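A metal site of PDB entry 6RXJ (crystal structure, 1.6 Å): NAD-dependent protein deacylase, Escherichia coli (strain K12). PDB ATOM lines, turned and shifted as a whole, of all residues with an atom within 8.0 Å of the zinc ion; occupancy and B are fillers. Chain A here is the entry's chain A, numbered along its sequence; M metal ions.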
ATOM      1  N   ARG A 129     -17.088   7.787   5.161  1.00  0.00           N
ATOM      2  CA  ARG A 129     -17.937   8.751   4.488  1.00  0.00           C
ATOM      3  C   ARG A 129     -19.137   8.037   3.912  1.00  0.00           C
ATOM      4  O   ARG A 129     -19.047   6.930   3.387  1.00  0.00           O
ATOM      5  CB  ARG A 129     -17.133   9.524   3.434  1.00  0.00           C
ATOM      6  CG  ARG A 129     -17.605   9.451   2.014  1.00  0.00           C
ATOM      7  CD  ARG A 129     -17.047  10.603   1.174  1.00  0.00           C
ATOM      8  NE  ARG A 129     -15.596  10.816   1.316  1.00  0.00           N
ATOM      9  CZ  ARG A 129     -14.726  10.800   0.309  1.00  0.00           C
ATOM     10  NH1 ARG A 129     -15.115  10.580  -0.947  1.00  0.00           N
ATOM     11  NH2 ARG A 129     -13.450  11.025   0.548  1.00  0.00           N
ATOM     12  N   CYS A 130     -20.296   8.677   4.064  1.00  0.00           N
ATOM     13  CA  CYS A 130     -21.505   8.206   3.425  1.00  0.00           C
ATOM     14  C   CYS A 130     -21.364   8.372   1.932  1.00  0.00           C
ATOM     15  O   CYS A 130     -21.076   9.467   1.457  1.00  0.00           O
ATOM     16  CB  CYS A 130     -22.706   8.977   3.923  1.00  0.00           C
ATOM     17  SG  CYS A 130     -24.221   8.486   3.047  1.00  0.00           S
ATOM     18  N   SER A 131     -21.559   7.286   1.201  1.00  0.00           N
ATOM     19  CA  SER A 131     -21.347   7.289  -0.242  1.00  0.00           C
ATOM     20  C   SER A 131     -22.423   8.089  -0.964  1.00  0.00           C
ATOM     21  O   SER A 131     -22.304   8.362  -2.151  1.00  0.00           O
ATOM     22  CB  SER A 131     -21.312   5.853  -0.766  1.00  0.00           C
ATOM     23  OG  SER A 131     -22.528   5.180  -0.483  1.00  0.00           O
ATOM     24  N   GLN A 132     -23.456   8.488  -0.241  1.00  0.00           N
ATOM     25  CA  GLN A 132     -24.605   9.176  -0.800  1.00  0.00           C
ATOM     26  C   GLN A 132     -24.568  10.678  -0.478  1.00  0.00           C
ATOM     27  O   GLN A 132     -24.669  11.515  -1.371  1.00  0.00           O
ATOM     28  CB  GLN A 132     -25.889   8.533  -0.249  1.00  0.00           C
ATOM     29  CG  GLN A 132     -27.183   8.840  -0.959  1.00  0.00           C
ATOM     30  CD  GLN A 132     -28.266   7.799  -0.655  1.00  0.00           C
ATOM     31  OE1 GLN A 132     -28.567   6.948  -1.494  1.00  0.00           O
ATOM     32  NE2 GLN A 132     -28.831   7.846   0.554  1.00  0.00           N
ATOM     33  N   SER A 133     -24.414  11.007   0.793  1.00  0.00           N
ATOM     34  CA  SER A 133     -24.481  12.402   1.258  1.00  0.00           C
ATOM     35  C   SER A 133     -23.120  13.081   1.339  1.00  0.00           C
ATOM     36  O   SER A 133     -23.030  14.316   1.367  1.00  0.00           O
ATOM     37  CB  SER A 133     -25.119  12.472   2.651  1.00  0.00           C
ATOM     38  OG  SER A 133     -24.199  12.069   3.667  1.00  0.00           O
ATOM     39  N   GLY A 134     -22.070  12.282   1.425  1.00  0.00           N
ATOM     40  CA  GLY A 134     -20.729  12.810   1.595  1.00  0.00           C
ATOM     41  C   GLY A 134     -20.415  13.216   3.020  1.00  0.00           C
ATOM     42  O   GLY A 134     -19.334  13.731   3.284  1.00  0.00           O
ATOM     43  N   GLN A 135     -21.335  12.996   3.940  1.00  0.00           N
ATOM     44  CA  GLN A 135     -21.081  13.325   5.332  1.00  0.00           C
ATOM     45  C   GLN A 135     -20.042  12.377   5.909  1.00  0.00           C
ATOM     46  O   GLN A 135     -20.002  11.204   5.566  1.00  0.00           O
ATOM     47  CB  GLN A 135     -22.374  13.277   6.147  1.00  0.00           C
ATOM     48  CG  GLN A 135     -23.301  14.434   5.830  1.00  0.00           C
ATOM     49  CD  GLN A 135     -24.414  14.572   6.833  1.00  0.00           C
ATOM     50  OE1 GLN A 135     -24.263  14.198   7.998  1.00  0.00           O
ATOM     51  NE2 GLN A 135     -25.548  15.120   6.391  1.00  0.00           N
ATOM     52  N   LEU A 137     -17.930  10.572   9.125  1.00  0.00           N
ATOM     53  CA  LEU A 137     -18.035  10.028  10.474  1.00  0.00           C
ATOM     54  C   LEU A 137     -16.667   9.611  10.998  1.00  0.00           C
ATOM     55  O   LEU A 137     -15.871   9.078  10.238  1.00  0.00           O
ATOM     56  CB  LEU A 137     -18.949   8.804  10.490  1.00  0.00           C
ATOM     57  CG  LEU A 137     -20.343   8.944   9.895  1.00  0.00           C
ATOM     58  CD1 LEU A 137     -20.971   7.564   9.713  1.00  0.00           C
ATOM     59  CD2 LEU A 137     -21.216   9.838  10.774  1.00  0.00           C
ATOM     60  N   LYS A 148     -24.116   0.804   7.374  1.00  0.00           N
ATOM     61  CA  LYS A 148     -24.722   1.818   6.534  1.00  0.00           C
ATOM     62  C   LYS A 148     -24.744   3.145   7.293  1.00  0.00           C
ATOM     63  O   LYS A 148     -24.540   3.167   8.506  1.00  0.00           O
ATOM     64  CB  LYS A 148     -26.138   1.425   6.132  1.00  0.00           C
ATOM     65  CG  LYS A 148     -26.228   0.070   5.435  1.00  0.00           C
ATOM     66  CD  LYS A 148     -26.103   0.198   3.920  1.00  0.00           C
ATOM     67  CE  LYS A 148     -26.307  -1.142   3.229  1.00  0.00           C
ATOM     68  NZ  LYS A 148     -27.656  -1.723   3.495  1.00  0.00           N
ATOM     69  N   CYS A 149     -24.985   4.230   6.581  1.00  0.00           N
ATOM     70  CA  CYS A 149     -24.951   5.547   7.185  1.00  0.00           C
ATOM     71  C   CYS A 149     -26.144   5.761   8.117  1.00  0.00           C
ATOM     72  O   CYS A 149     -27.080   4.962   8.135  1.00  0.00           O
ATOM     73  CB  CYS A 149     -24.939   6.626   6.121  1.00  0.00           C
ATOM     74  SG  CYS A 149     -26.595   6.928   5.395  1.00  0.00           S
ATOM     75  N   HIS A 150     -26.098   6.829   8.894  1.00  0.00           N
ATOM     76  CA  HIS A 150     -27.271   7.231   9.668  1.00  0.00           C
ATOM     77  C   HIS A 150     -27.616   8.674   9.351  1.00  0.00           C
ATOM     78  O   HIS A 150     -28.299   9.342  10.124  1.00  0.00           O
ATOM     79  CB  HIS A 150     -27.052   7.027  11.170  1.00  0.00           C
ATOM     80  CG  HIS A 150     -25.757   7.551  11.690  1.00  0.00           C
ATOM     81  ND1 HIS A 150     -25.568   8.872  12.049  1.00  0.00           N
ATOM     82  CD2 HIS A 150     -24.579   6.918  11.913  1.00  0.00           C
ATOM     83  CE1 HIS A 150     -24.330   9.024  12.477  1.00  0.00           C
ATOM     84  NE2 HIS A 150     -23.707   7.858  12.403  1.00  0.00           N
ATOM     85  N   CYS A 151     -27.155   9.144   8.192  1.00  0.00           N
ATOM     86  CA  CYS A 151     -27.413  10.528   7.788  1.00  0.00           C
ATOM     87  C   CYS A 151     -28.489  10.627   6.705  1.00  0.00           C
ATOM     88  O   CYS A 151     -28.898  11.730   6.351  1.00  0.00           O
ATOM     89  CB  CYS A 151     -26.118  11.198   7.317  1.00  0.00           C
ATOM     90  SG  CYS A 151     -25.074  10.310   6.109  1.00  0.00           S
ATOM     91  N   CYS A 152     -28.929   9.487   6.187  1.00  0.00           N
ATOM     92  CA  CYS A 152     -29.862   9.440   5.055  1.00  0.00           C
ATOM     93  C   CYS A 152     -31.147   8.705   5.407  1.00  0.00           C
ATOM     94  O   CYS A 152     -31.126   7.716   6.130  1.00  0.00           O
ATOM     95  CB  CYS A 152     -29.216   8.766   3.848  1.00  0.00           C
ATOM     96  SG  CYS A 152     -27.833   9.678   3.130  1.00  0.00           S
ATOM     97  N   GLN A 153     -32.255   9.160   4.842  1.00  0.00           N
ATOM     98  CA  GLN A 153     -33.517   8.457   5.038  1.00  0.00           C
ATOM     99  C   GLN A 153     -33.400   7.020   4.544  1.00  0.00           C
ATOM    100  O   GLN A 153     -33.848   6.081   5.205  1.00  0.00           O
ATOM    101  CB  GLN A 153     -34.657   9.168   4.308  1.00  0.00           C
ATOM    102  CG  GLN A 153     -35.961   8.379   4.334  1.00  0.00           C
ATOM    103  CD  GLN A 153     -37.118   9.210   3.798  1.00  0.00           C
ATOM    104  OE1 GLN A 153     -37.157  10.416   4.005  1.00  0.00           O
ATOM    105  NE2 GLN A 153     -38.048   8.565   3.118  1.00  0.00           N
ATOM    106  N   PHE A 154     -32.805   6.864   3.364  1.00  0.00           N
ATOM    107  CA  PHE A 154     -32.482   5.556   2.833  1.00  0.00           C
ATOM    108  C   PHE A 154     -31.000   5.282   3.095  1.00  0.00           C
ATOM    109  O   PHE A 154     -30.160   5.819   2.377  1.00  0.00           O
ATOM    110  CB  PHE A 154     -32.774   5.466   1.347  1.00  0.00           C
ATOM    111  CG  PHE A 154     -34.210   5.758   0.997  1.00  0.00           C
ATOM    112  CD1 PHE A 154     -35.163   4.752   1.020  1.00  0.00           C
ATOM    113  CD2 PHE A 154     -34.601   7.039   0.639  1.00  0.00           C
ATOM    114  CE1 PHE A 154     -36.477   5.029   0.684  1.00  0.00           C
ATOM    115  CE2 PHE A 154     -35.904   7.310   0.309  1.00  0.00           C
ATOM    116  CZ  PHE A 154     -36.844   6.304   0.327  1.00  0.00           C
ATOM    117  N   PRO A 155     -30.684   4.472   4.109  1.00  0.00           N
ATOM    118  CA  PRO A 155     -29.270   4.303   4.501  1.00  0.00           C
ATOM    119  C   PRO A 155     -28.399   3.836   3.340  1.00  0.00           C
ATOM    120  O   PRO A 155     -28.803   2.957   2.583  1.00  0.00           O
ATOM    121  CB  PRO A 155     -29.337   3.231   5.600  1.00  0.00           C
ATOM    122  CG  PRO A 155     -30.733   3.312   6.119  1.00  0.00           C
ATOM    123  CD  PRO A 155     -31.582   3.650   4.947  1.00  0.00           C
ATOM    124  N   ALA A 156     -27.203   4.420   3.218  1.00  0.00           N
ATOM    125  CA  ALA A 156     -26.305   4.107   2.106  1.00  0.00           C
ATOM    126  C   ALA A 156     -25.017   3.481   2.631  1.00  0.00           C
ATOM    127  O   ALA A 156     -24.677   3.655   3.792  1.00  0.00           O
ATOM    128  CB  ALA A 156     -26.004   5.349   1.316  1.00  0.00           C
ATOM    129  N   PRO A 157     -24.288   2.744   1.767  1.00  0.00           N
ATOM    130  CA  PRO A 157     -23.024   2.135   2.168  1.00  0.00           C
ATOM    131  C   PRO A 157     -21.980   3.176   2.562  1.00  0.00           C
ATOM    132  O   PRO A 157     -21.981   4.303   2.048  1.00  0.00           O
ATOM    133  CB  PRO A 157     -22.569   1.377   0.911  1.00  0.00           C
ATOM    134  CG  PRO A 157     -23.763   1.227   0.092  1.00  0.00           C
ATOM    135  CD  PRO A 157     -24.641   2.403   0.376  1.00  0.00           C
ATOM    136  N   LEU A 158     -21.082   2.777   3.456  1.00  0.00           N
ATOM    137  CA  LEU A 158     -19.984   3.620   3.911  1.00  0.00           C
ATOM    138  C   LEU A 158     -18.722   3.259   3.149  1.00  0.00           C
ATOM    139  O   LEU A 158     -18.495   2.098   2.843  1.00  0.00           O
ATOM    140  CB  LEU A 158     -19.749   3.445   5.415  1.00  0.00           C
ATOM    141  CG  LEU A 158     -20.928   3.828   6.314  1.00  0.00           C
ATOM    142  CD1 LEU A 158     -20.665   3.430   7.750  1.00  0.00           C
ATOM    143  CD2 LEU A 158     -21.218   5.311   6.211  1.00  0.00           C
HETATM  144 ZN    ZN M   1     -26.078   8.931   4.392  1.00  0.00          ZN
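SG of Cys 152 binds the zinc ion (2.3 Å). SG of Cys 149 is bound to the zinc ion (2.3 Å). SG of Cys 130 binds the zinc ion. SG of Cys 151 is bound to the zinc ion (2.4 Å).
The backbone NH (N) of Ser 133 sits close to the side-chain sulfur (SG) of Cys 130 (3.4 Å). The side-chain sulfur of Cys 152 lies close to the side-chain amide nitrogen of Gln 132, at 3.3 Å. The backbone carbonyl oxygen (O) of Gln 135 is in hydrogen-bond range of the backbone NH (N) of Cys 130 (3.0 Å). The side-chain sulfur (SG) of Cys 151 lies close to the side-chain hydroxyl (OG) of Ser 133 (3.1 Å). The side-chain sulfur (SG) of Cys 130 sits close to the backbone NH (N) of Gln 132. N of Gln 135 is in hydrogen-bond range of OG of Ser 133 (3.0 Å). N of Cys 149 is in hydrogen-bond range of O of Ala 156, 2.9 Å away.
Residues that only touch the zinc ion: Ser 133. Five residues have an atom within 4 Å of the zinc ion: Cys 130, Ser 133, Cys 149, Cys 151 and Cys 152. The nearest printed residue that does not touch the zinc ion is Gln 132 (4.7 Å).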
